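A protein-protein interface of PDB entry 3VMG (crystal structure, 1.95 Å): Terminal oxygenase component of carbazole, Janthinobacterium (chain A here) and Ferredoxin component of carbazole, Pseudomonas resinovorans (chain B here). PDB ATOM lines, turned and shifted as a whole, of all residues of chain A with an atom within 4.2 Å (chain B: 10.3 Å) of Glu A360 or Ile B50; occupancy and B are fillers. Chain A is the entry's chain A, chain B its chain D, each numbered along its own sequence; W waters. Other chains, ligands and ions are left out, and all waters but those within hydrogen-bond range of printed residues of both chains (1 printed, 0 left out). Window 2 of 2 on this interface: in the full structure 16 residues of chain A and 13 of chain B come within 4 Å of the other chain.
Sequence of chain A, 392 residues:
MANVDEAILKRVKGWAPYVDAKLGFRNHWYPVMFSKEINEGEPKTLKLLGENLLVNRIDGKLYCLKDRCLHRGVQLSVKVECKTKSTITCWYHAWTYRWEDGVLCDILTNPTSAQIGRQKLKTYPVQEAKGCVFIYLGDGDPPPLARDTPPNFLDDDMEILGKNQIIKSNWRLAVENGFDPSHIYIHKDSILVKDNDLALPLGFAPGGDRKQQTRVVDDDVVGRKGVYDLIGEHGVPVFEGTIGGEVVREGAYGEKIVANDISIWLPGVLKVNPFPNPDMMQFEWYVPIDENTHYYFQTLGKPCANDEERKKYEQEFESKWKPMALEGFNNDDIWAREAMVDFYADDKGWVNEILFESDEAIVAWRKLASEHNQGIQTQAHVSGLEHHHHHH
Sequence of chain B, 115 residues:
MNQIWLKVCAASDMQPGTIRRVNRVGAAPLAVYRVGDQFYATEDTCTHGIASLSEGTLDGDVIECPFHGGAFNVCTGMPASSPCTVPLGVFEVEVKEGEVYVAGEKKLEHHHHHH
Hydrophobic or aromatic side chains of chain A that line the printed part of chain B: Val A363. Printed residues of chain B that touch a printed residue of chain A: Arg B21, Gly B49, Ile B50, Glu B55 and Phe B67. Hydrophobic or aromatic side chains of chain B within 4 Å of the printed part of chain A: Ile B50 and Phe B67. Along chain B the printed residues that touch a printed residue of chain A span positions 21 to 67. Among the printed residues, 7 pairs touch across the chains.
NH1 of Arg B21 lies within salt-bridge range of OD2 of Asp B44 (3.9 Å). The backbone NH of Phe B67 lies close to the side-chain sulfur of Cys B65 (3.5 Å). N of Phe A356 sits at hydrogen-bond distance from OD2 of Asp A359 (2.9 Å).
The guanidinium group (NH2) of Arg A210 lies within salt-bridge range of the side-chain carboxylate (OE2) of Glu B55 (3.1 Å).
Among the printed residues, pairs that only touch across the chains: Arg A210 with Arg B21 (3.9 Å), Leu A355 with Gly B49 (3.6 Å), Phe A356 with Ile B50 (3.6 Å), Glu A357 with Ile B50 (3.9 Å), Glu A360 with Ile B50 (3.6 Å) and Val A363 with Phe B67 (3.9 Å).
Water W1 bridges O of His B48 (2.7 Å) and N of Leu A355 (2.8 Å).
Glu A360 touches just one residue of chain B: Ile B50 (3.6 Å). Printed residues of chain A within 4 Å of Ile B50: Phe A356, Glu A357 and Glu A360. No residue of chain B comes within 4 Å of Ala A361. Val A363 touches just one residue of chain B: Phe B67 (3.9 Å). Of the printed residues of chain A, Glu B55 touches Arg A210. Printed residues of chain B within 4 Å of Leu A355: Gly B49 (3.6 Å). The nearest residue of chain B that does not touch Glu A360 is Phe B67 (6.0 Å). The nearest printed residue of chain A that does not touch Ile B50 is Asp A359 (4.03 Å).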
ATOM      1  N   ARG A 210      24.266 -21.406   2.810  1.00  0.00           N
ATOM      2  CA  ARG A 210      23.575 -21.189   1.525  1.00  0.00           C
ATOM      3  C   ARG A 210      24.365 -21.758   0.340  1.00  0.00           C
ATOM      4  O   ARG A 210      23.823 -22.381  -0.568  1.00  0.00           O
ATOM      5  CB  ARG A 210      23.305 -19.689   1.315  1.00  0.00           C
ATOM      6  CG  ARG A 210      22.847 -19.386  -0.122  1.00  0.00           C
ATOM      7  CD  ARG A 210      22.252 -17.965  -0.305  1.00  0.00           C
ATOM      8  NE  ARG A 210      23.322 -16.956  -0.397  1.00  0.00           N
ATOM      9  CZ  ARG A 210      23.024 -15.700  -0.760  1.00  0.00           C
ATOM     10  NH1 ARG A 210      21.805 -15.382  -1.143  1.00  0.00           N
ATOM     11  NH2 ARG A 210      23.862 -14.724  -0.407  1.00  0.00           N
ATOM     12  N   LEU A 355       9.375 -16.457  -0.961  1.00  0.00           N
ATOM     13  CA  LEU A 355      10.149 -17.694  -0.962  1.00  0.00           C
ATOM     14  C   LEU A 355      10.635 -18.112   0.413  1.00  0.00           C
ATOM     15  O   LEU A 355      10.661 -17.299   1.335  1.00  0.00           O
ATOM     16  CB  LEU A 355      11.361 -17.541  -1.884  1.00  0.00           C
ATOM     17  CG  LEU A 355      11.097 -16.933  -3.268  1.00  0.00           C
ATOM     18  CD1 LEU A 355      12.402 -16.855  -4.034  1.00  0.00           C
ATOM     19  CD2 LEU A 355      10.079 -17.784  -4.034  1.00  0.00           C
ATOM     20  N   PHE A 356      10.969 -19.392   0.567  1.00  0.00           N
ATOM     21  CA  PHE A 356      11.532 -19.839   1.829  1.00  0.00           C
ATOM     22  C   PHE A 356      12.826 -20.596   1.549  1.00  0.00           C
ATOM     23  O   PHE A 356      13.262 -20.683   0.390  1.00  0.00           O
ATOM     24  CB  PHE A 356      10.509 -20.597   2.723  1.00  0.00           C
ATOM     25  CG  PHE A 356      10.161 -22.004   2.298  1.00  0.00           C
ATOM     26  CD1 PHE A 356      10.031 -22.364   0.958  1.00  0.00           C
ATOM     27  CD2 PHE A 356       9.839 -22.950   3.277  1.00  0.00           C
ATOM     28  CE1 PHE A 356       9.579 -23.639   0.599  1.00  0.00           C
ATOM     29  CE2 PHE A 356       9.384 -24.232   2.931  1.00  0.00           C
ATOM     30  CZ  PHE A 356       9.252 -24.576   1.587  1.00  0.00           C
ATOM     31  N   GLU A 357      13.454 -21.118   2.595  1.00  0.00           N
ATOM     32  CA  GLU A 357      14.757 -21.764   2.463  1.00  0.00           C
ATOM     33  C   GLU A 357      15.081 -22.690   1.291  1.00  0.00           C
ATOM     34  O   GLU A 357      16.074 -22.462   0.605  1.00  0.00           O
ATOM     35  CB  GLU A 357      15.124 -22.464   3.777  1.00  0.00           C
ATOM     36  CG  GLU A 357      15.377 -21.512   4.947  1.00  0.00           C
ATOM     37  CD  GLU A 357      14.100 -21.011   5.611  1.00  0.00           C
ATOM     38  OE1 GLU A 357      12.997 -21.446   5.216  1.00  0.00           O
ATOM     39  OE2 GLU A 357      14.203 -20.175   6.538  1.00  0.00           O
ATOM     40  N   SER A 358      14.275 -23.722   1.058  1.00  0.00           N
ATOM     41  CA  SER A 358      14.556 -24.658  -0.031  1.00  0.00           C
ATOM     42  C   SER A 358      14.543 -24.017  -1.411  1.00  0.00           C
ATOM     43  O   SER A 358      15.028 -24.609  -2.375  1.00  0.00           O
ATOM     44  CB  SER A 358      13.576 -25.849   0.004  1.00  0.00           C
ATOM     45  OG  SER A 358      12.221 -25.435  -0.074  1.00  0.00           O
ATOM     46  N   ASP A 359      13.994 -22.810  -1.514  1.00  0.00           N
ATOM     47  CA  ASP A 359      13.954 -22.122  -2.798  1.00  0.00           C
ATOM     48  C   ASP A 359      15.334 -21.614  -3.218  1.00  0.00           C
ATOM     49  O   ASP A 359      15.474 -20.990  -4.264  1.00  0.00           O
ATOM     50  CB  ASP A 359      12.944 -20.963  -2.771  1.00  0.00           C
ATOM     51  CG  ASP A 359      11.507 -21.452  -2.688  1.00  0.00           C
ATOM     52  OD1 ASP A 359      11.175 -22.429  -3.397  1.00  0.00           O
ATOM     53  OD2 ASP A 359      10.712 -20.863  -1.929  1.00  0.00           O
ATOM     54  N   GLU A 360      16.351 -21.874  -2.400  1.00  0.00           N
ATOM     55  CA  GLU A 360      17.713 -21.472  -2.755  1.00  0.00           C
ATOM     56  C   GLU A 360      18.048 -22.191  -4.061  1.00  0.00           C
ATOM     57  O   GLU A 360      18.777 -21.672  -4.897  1.00  0.00           O
ATOM     58  CB  GLU A 360      18.725 -21.907  -1.685  1.00  0.00           C
ATOM     59  CG  GLU A 360      18.743 -21.065  -0.422  1.00  0.00           C
ATOM     60  CD  GLU A 360      19.251 -19.644  -0.656  1.00  0.00           C
ATOM     61  OE1 GLU A 360      19.725 -19.345  -1.781  1.00  0.00           O
ATOM     62  OE2 GLU A 360      19.187 -18.829   0.294  1.00  0.00           O
ATOM     63  N   ALA A 361      17.507 -23.398  -4.220  1.00  0.00           N
ATOM     64  CA  ALA A 361      17.748 -24.191  -5.420  1.00  0.00           C
ATOM     65  C   ALA A 361      17.145 -23.498  -6.647  1.00  0.00           C
ATOM     66  O   ALA A 361      17.764 -23.433  -7.703  1.00  0.00           O
ATOM     67  CB  ALA A 361      17.141 -25.583  -5.252  1.00  0.00           C
ATOM     68  N   ILE A 362      15.931 -22.983  -6.502  1.00  0.00           N
ATOM     69  CA  ILE A 362      15.272 -22.296  -7.600  1.00  0.00           C
ATOM     70  C   ILE A 362      16.008 -20.998  -7.936  1.00  0.00           C
ATOM     71  O   ILE A 362      16.214 -20.680  -9.103  1.00  0.00           O
ATOM     72  CB  ILE A 362      13.798 -22.018  -7.256  1.00  0.00           C
ATOM     73  CG1 ILE A 362      13.010 -23.339  -7.340  1.00  0.00           C
ATOM     74  CG2 ILE A 362      13.218 -20.956  -8.198  1.00  0.00           C
ATOM     75  CD1 ILE A 362      11.568 -23.252  -6.839  1.00  0.00           C
ATOM     76  N   VAL A 363      16.414 -20.256  -6.912  1.00  0.00           N
ATOM     77  CA  VAL A 363      17.140 -19.011  -7.135  1.00  0.00           C
ATOM     78  C   VAL A 363      18.453 -19.271  -7.874  1.00  0.00           C
ATOM     79  O   VAL A 363      18.835 -18.504  -8.753  1.00  0.00           O
ATOM     80  CB  VAL A 363      17.439 -18.292  -5.797  1.00  0.00           C
ATOM     81  CG1 VAL A 363      18.560 -17.263  -5.982  1.00  0.00           C
ATOM     82  CG2 VAL A 363      16.177 -17.604  -5.305  1.00  0.00           C
ATOM     83  N   ALA A 364      19.146 -20.350  -7.523  1.00  0.00           N
ATOM     84  CA  ALA A 364      20.406 -20.670  -8.192  1.00  0.00           C
ATOM     85  C   ALA A 364      20.169 -20.966  -9.673  1.00  0.00           C
ATOM     86  O   ALA A 364      20.992 -20.611 -10.523  1.00  0.00           O
ATOM     87  CB  ALA A 364      21.083 -21.863  -7.518  1.00  0.00           C
ATOM     88  N   ARG B  21      28.076  -6.749   5.194  1.00  0.00           N
ATOM     89  CA  ARG B  21      27.417  -7.890   5.818  1.00  0.00           C
ATOM     90  C   ARG B  21      28.230  -8.444   6.979  1.00  0.00           C
ATOM     91  O   ARG B  21      29.450  -8.577   6.888  1.00  0.00           O
ATOM     92  CB  ARG B  21      27.181  -9.001   4.791  1.00  0.00           C
ATOM     93  CG  ARG B  21      26.656 -10.293   5.403  1.00  0.00           C
ATOM     94  CD  ARG B  21      26.308 -11.325   4.343  1.00  0.00           C
ATOM     95  NE  ARG B  21      26.055 -12.635   4.938  1.00  0.00           N
ATOM     96  CZ  ARG B  21      25.496 -13.657   4.296  1.00  0.00           C
ATOM     97  NH1 ARG B  21      25.126 -13.526   3.028  1.00  0.00           N
ATOM     98  NH2 ARG B  21      25.306 -14.810   4.923  1.00  0.00           N
ATOM     99  N   PRO B  29      22.747 -13.763   9.758  1.00  0.00           N
ATOM    100  CA  PRO B  29      23.601 -12.613   9.436  1.00  0.00           C
ATOM    101  C   PRO B  29      22.932 -11.249   9.608  1.00  0.00           C
ATOM    102  O   PRO B  29      21.707 -11.124   9.569  1.00  0.00           O
ATOM    103  CB  PRO B  29      24.002 -12.881   7.989  1.00  0.00           C
ATOM    104  CG  PRO B  29      22.804 -13.595   7.444  1.00  0.00           C
ATOM    105  CD  PRO B  29      22.482 -14.568   8.551  1.00  0.00           C
ATOM    106  N   GLU B  43      18.718  -7.062  10.437  1.00  0.00           N
ATOM    107  CA  GLU B  43      19.011  -8.426  10.034  1.00  0.00           C
ATOM    108  C   GLU B  43      19.316  -8.323   8.539  1.00  0.00           C
ATOM    109  O   GLU B  43      18.787  -7.443   7.854  1.00  0.00           O
ATOM    110  CB  GLU B  43      17.816  -9.350  10.323  1.00  0.00           C
ATOM    111  CG  GLU B  43      16.481  -8.928   9.736  1.00  0.00           C
ATOM    112  CD  GLU B  43      15.321  -9.769  10.273  1.00  0.00           C
ATOM    113  OE1 GLU B  43      15.465 -11.010  10.346  1.00  0.00           O
ATOM    114  OE2 GLU B  43      14.263  -9.192  10.616  1.00  0.00           O
ATOM    115  N   ASP B  44      20.195  -9.186   8.042  1.00  0.00           N
ATOM    116  CA  ASP B  44      20.571  -9.154   6.633  1.00  0.00           C
ATOM    117  C   ASP B  44      19.526  -9.745   5.689  1.00  0.00           C
ATOM    118  O   ASP B  44      19.401  -9.320   4.542  1.00  0.00           O
ATOM    119  CB  ASP B  44      21.892  -9.893   6.420  1.00  0.00           C
ATOM    120  CG  ASP B  44      22.330  -9.879   4.971  1.00  0.00           C
ATOM    121  OD1 ASP B  44      22.505  -8.768   4.428  1.00  0.00           O
ATOM    122  OD2 ASP B  44      22.495 -10.969   4.372  1.00  0.00           O
ATOM    123  N   THR B  45      18.783 -10.730   6.172  1.00  0.00           N
ATOM    124  CA  THR B  45      17.778 -11.378   5.343  1.00  0.00           C
ATOM    125  C   THR B  45      16.514 -10.547   5.172  1.00  0.00           C
ATOM    126  O   THR B  45      15.903 -10.104   6.146  1.00  0.00           O
ATOM    127  CB  THR B  45      17.400 -12.745   5.922  1.00  0.00           C
ATOM    128  OG1 THR B  45      18.595 -13.504   6.154  1.00  0.00           O
ATOM    129  CG2 THR B  45      16.501 -13.503   4.947  1.00  0.00           C
ATOM    130  N   CYS B  46      16.129 -10.333   3.918  1.00  0.00           N
ATOM    131  CA  CYS B  46      14.922  -9.571   3.615  1.00  0.00           C
ATOM    132  C   CYS B  46      13.734 -10.306   4.241  1.00  0.00           C
ATOM    133  O   CYS B  46      13.678 -11.534   4.200  1.00  0.00           O
ATOM    134  CB  CYS B  46      14.744  -9.465   2.099  1.00  0.00           C
ATOM    135  SG  CYS B  46      13.335  -8.480   1.602  1.00  0.00           S
ATOM    136  N   THR B  47      12.798  -9.563   4.825  1.00  0.00           N
ATOM    137  CA  THR B  47      11.632 -10.178   5.462  1.00  0.00           C
ATOM    138  C   THR B  47      10.623 -10.727   4.454  1.00  0.00           C
ATOM    139  O   THR B  47       9.691 -11.448   4.825  1.00  0.00           O
ATOM    140  CB  THR B  47      10.890  -9.176   6.390  1.00  0.00           C
ATOM    141  OG1 THR B  47      10.336  -8.110   5.610  1.00  0.00           O
ATOM    142  CG2 THR B  47      11.845  -8.596   7.427  1.00  0.00           C
ATOM    143  N   HIS B  48      10.810 -10.392   3.182  1.00  0.00           N
ATOM    144  CA  HIS B  48       9.905 -10.846   2.127  1.00  0.00           C
ATOM    145  C   HIS B  48      10.327 -12.178   1.501  1.00  0.00           C
ATOM    146  O   HIS B  48       9.588 -12.756   0.704  1.00  0.00           O
ATOM    147  CB  HIS B  48       9.802  -9.767   1.040  1.00  0.00           C
ATOM    148  CG  HIS B  48       8.943 -10.152  -0.129  1.00  0.00           C
ATOM    149  ND1 HIS B  48       9.469 -10.495  -1.359  1.00  0.00           N
ATOM    150  CD2 HIS B  48       7.598 -10.246  -0.256  1.00  0.00           C
ATOM    151  CE1 HIS B  48       8.483 -10.784  -2.191  1.00  0.00           C
ATOM    152  NE2 HIS B  48       7.339 -10.640  -1.547  1.00  0.00           N
ATOM    153  N   GLY B  49      11.511 -12.665   1.857  1.00  0.00           N
ATOM    154  CA  GLY B  49      11.975 -13.918   1.289  1.00  0.00           C
ATOM    155  C   GLY B  49      13.306 -14.396   1.829  1.00  0.00           C
ATOM    156  O   GLY B  49      13.494 -14.477   3.040  1.00  0.00           O
ATOM    157  N   ILE B  50      14.236 -14.715   0.935  1.00  0.00           N
ATOM    158  CA  ILE B  50      15.550 -15.201   1.353  1.00  0.00           C
ATOM    159  C   ILE B  50      16.715 -14.384   0.798  1.00  0.00           C
ATOM    160  O   ILE B  50      17.859 -14.835   0.805  1.00  0.00           O
ATOM    161  CB  ILE B  50      15.742 -16.673   0.938  1.00  0.00           C
ATOM    162  CG1 ILE B  50      15.622 -16.813  -0.581  1.00  0.00           C
ATOM    163  CG2 ILE B  50      14.698 -17.537   1.624  1.00  0.00           C
ATOM    164  CD1 ILE B  50      15.880 -18.233  -1.098  1.00  0.00           C
ATOM    165  N   ALA B  51      16.432 -13.179   0.319  1.00  0.00           N
ATOM    166  CA  ALA B  51      17.488 -12.332  -0.231  1.00  0.00           C
ATOM    167  C   ALA B  51      18.401 -11.742   0.845  1.00  0.00           C
ATOM    168  O   ALA B  51      18.003 -11.586   1.998  1.00  0.00           O
ATOM    169  CB  ALA B  51      16.872 -11.203  -1.042  1.00  0.00           C
ATOM    170  N   SER B  52      19.633 -11.427   0.454  1.00  0.00           N
ATOM    171  CA  SER B  52      20.590 -10.801   1.357  1.00  0.00           C
ATOM    172  C   SER B  52      20.596  -9.307   1.032  1.00  0.00           C
ATOM    173  O   SER B  52      21.004  -8.909  -0.058  1.00  0.00           O
ATOM    174  CB  SER B  52      21.993 -11.370   1.145  1.00  0.00           C
ATOM    175  OG  SER B  52      22.959 -10.558   1.793  1.00  0.00           O
ATOM    176  N   LEU B  53      20.138  -8.490   1.977  1.00  0.00           N
ATOM    177  CA  LEU B  53      20.075  -7.043   1.784  1.00  0.00           C
ATOM    178  C   LEU B  53      21.445  -6.399   1.584  1.00  0.00           C
ATOM    179  O   LEU B  53      21.558  -5.362   0.927  1.00  0.00           O
ATOM    180  CB  LEU B  53      19.360  -6.386   2.971  1.00  0.00           C
ATOM    181  CG  LEU B  53      17.870  -6.725   3.095  1.00  0.00           C
ATOM    182  CD1 LEU B  53      17.296  -6.124   4.369  1.00  0.00           C
ATOM    183  CD2 LEU B  53      17.129  -6.199   1.872  1.00  0.00           C
ATOM    184  N   SER B  54      22.485  -7.012   2.143  1.00  0.00           N
ATOM    185  CA  SER B  54      23.831  -6.467   2.001  1.00  0.00           C
ATOM    186  C   SER B  54      24.258  -6.472   0.529  1.00  0.00           C
ATOM    187  O   SER B  54      25.233  -5.815   0.151  1.00  0.00           O
ATOM    188  CB  SER B  54      24.820  -7.257   2.866  1.00  0.00           C
ATOM    189  OG  SER B  54      24.883  -8.617   2.481  1.00  0.00           O
ATOM    190  N   GLU B  55      23.521  -7.204  -0.305  1.00  0.00           N
ATOM    191  CA  GLU B  55      23.821  -7.250  -1.732  1.00  0.00           C
ATOM    192  C   GLU B  55      22.878  -6.310  -2.479  1.00  0.00           C
ATOM    193  O   GLU B  55      22.834  -6.305  -3.708  1.00  0.00           O
ATOM    194  CB  GLU B  55      23.685  -8.679  -2.272  1.00  0.00           C
ATOM    195  CG  GLU B  55      24.816  -9.605  -1.835  1.00  0.00           C
ATOM    196  CD  GLU B  55      24.637 -11.037  -2.314  1.00  0.00           C
ATOM    197  OE1 GLU B  55      24.443 -11.242  -3.532  1.00  0.00           O
ATOM    198  OE2 GLU B  55      24.701 -11.961  -1.471  1.00  0.00           O
ATOM    199  N   CYS B  65      16.033  -4.207  -1.683  1.00  0.00           N
ATOM    200  CA  CYS B  65      16.359  -5.622  -1.828  1.00  0.00           C
ATOM    201  C   CYS B  65      16.617  -5.975  -3.298  1.00  0.00           C
ATOM    202  O   CYS B  65      15.873  -5.561  -4.181  1.00  0.00           O
ATOM    203  CB  CYS B  65      15.212  -6.471  -1.279  1.00  0.00           C
ATOM    204  SG  CYS B  65      15.431  -8.233  -1.527  1.00  0.00           S
ATOM    205  N   PRO B  66      17.677  -6.757  -3.570  1.00  0.00           N
ATOM    206  CA  PRO B  66      18.062  -7.177  -4.924  1.00  0.00           C
ATOM    207  C   PRO B  66      17.152  -8.205  -5.599  1.00  0.00           C
ATOM    208  O   PRO B  66      17.203  -8.376  -6.820  1.00  0.00           O
ATOM    209  CB  PRO B  66      19.471  -7.718  -4.716  1.00  0.00           C
ATOM    210  CG  PRO B  66      19.363  -8.357  -3.376  1.00  0.00           C
ATOM    211  CD  PRO B  66      18.619  -7.303  -2.576  1.00  0.00           C
ATOM    212  N   PHE B  67      16.317  -8.885  -4.821  1.00  0.00           N
ATOM    213  CA  PHE B  67      15.446  -9.901  -5.399  1.00  0.00           C
ATOM    214  C   PHE B  67      14.146  -9.393  -6.017  1.00  0.00           C
ATOM    215  O   PHE B  67      13.878  -9.662  -7.187  1.00  0.00           O
ATOM    216  CB  PHE B  67      15.155 -10.994  -4.360  1.00  0.00           C
ATOM    217  CG  PHE B  67      16.251 -12.029  -4.240  1.00  0.00           C
ATOM    218  CD1 PHE B  67      17.549 -11.747  -4.656  1.00  0.00           C
ATOM    219  CD2 PHE B  67      15.985 -13.280  -3.688  1.00  0.00           C
ATOM    220  CE1 PHE B  67      18.571 -12.697  -4.522  1.00  0.00           C
ATOM    221  CE2 PHE B  67      16.997 -14.235  -3.548  1.00  0.00           C
ATOM    222  CZ  PHE B  67      18.288 -13.947  -3.963  1.00  0.00           C
ATOM    223  N   HIS B  68      13.336  -8.660  -5.257  1.00  0.00           N
ATOM    224  CA  HIS B  68      12.074  -8.173  -5.807  1.00  0.00           C
ATOM    225  C   HIS B  68      11.888  -6.660  -5.763  1.00  0.00           C
ATOM    226  O   HIS B  68      10.844  -6.147  -6.157  1.00  0.00           O
ATOM    227  CB  HIS B  68      10.898  -8.862  -5.112  1.00  0.00           C
ATOM    228  CG  HIS B  68      10.977 -10.359  -5.140  1.00  0.00           C
ATOM    229  ND1 HIS B  68      11.222 -11.111  -4.012  1.00  0.00           N
ATOM    230  CD2 HIS B  68      10.866 -11.241  -6.162  1.00  0.00           C
ATOM    231  CE1 HIS B  68      11.257 -12.392  -4.335  1.00  0.00           C
ATOM    232  NE2 HIS B  68      11.044 -12.500  -5.635  1.00  0.00           N
ATOM    233  N   PHE B  72      13.432  -1.038   2.742  1.00  0.00           N
ATOM    234  CA  PHE B  72      13.261  -0.756   4.162  1.00  0.00           C
ATOM    235  C   PHE B  72      14.043   0.486   4.568  1.00  0.00           C
ATOM    236  O   PHE B  72      15.079   0.793   3.985  1.00  0.00           O
ATOM    237  CB  PHE B  72      13.798  -1.915   5.008  1.00  0.00           C
ATOM    238  CG  PHE B  72      13.117  -3.231   4.766  1.00  0.00           C
ATOM    239  CD1 PHE B  72      11.917  -3.534   5.395  1.00  0.00           C
ATOM    240  CD2 PHE B  72      13.692  -4.179   3.924  1.00  0.00           C
ATOM    241  CE1 PHE B  72      11.295  -4.766   5.196  1.00  0.00           C
ATOM    242  CE2 PHE B  72      13.080  -5.417   3.716  1.00  0.00           C
ATOM    243  CZ  PHE B  72      11.879  -5.709   4.353  1.00  0.00           C
ATOM    244  N   CYS B  84       7.523  -5.714   0.249  1.00  0.00           N
ATOM    245  CA  CYS B  84       7.799  -5.879   1.674  1.00  0.00           C
ATOM    246  C   CYS B  84       6.700  -5.299   2.563  1.00  0.00           C
ATOM    247  O   CYS B  84       6.147  -4.234   2.271  1.00  0.00           O
ATOM    248  CB  CYS B  84       9.141  -5.237   2.027  1.00  0.00           C
ATOM    249  SG  CYS B  84      10.550  -6.032   1.232  1.00  0.00           S
ATOM    250  N   LEU B  88      11.693  -5.052   9.490  1.00  0.00           N
ATOM    251  CA  LEU B  88      12.971  -5.729   9.620  1.00  0.00           C
ATOM    252  C   LEU B  88      13.434  -5.579  11.071  1.00  0.00           C
ATOM    253  O   LEU B  88      13.097  -4.599  11.737  1.00  0.00           O
ATOM    254  CB  LEU B  88      13.975  -5.077   8.659  1.00  0.00           C
ATOM    255  CG  LEU B  88      15.246  -5.784   8.184  1.00  0.00           C
ATOM    256  CD1 LEU B  88      14.903  -7.070   7.460  1.00  0.00           C
ATOM    257  CD2 LEU B  88      16.002  -4.847   7.246  1.00  0.00           C
HETATM  258  O   HOH W   1      10.179 -13.870  -1.701  1.00  0.00           O
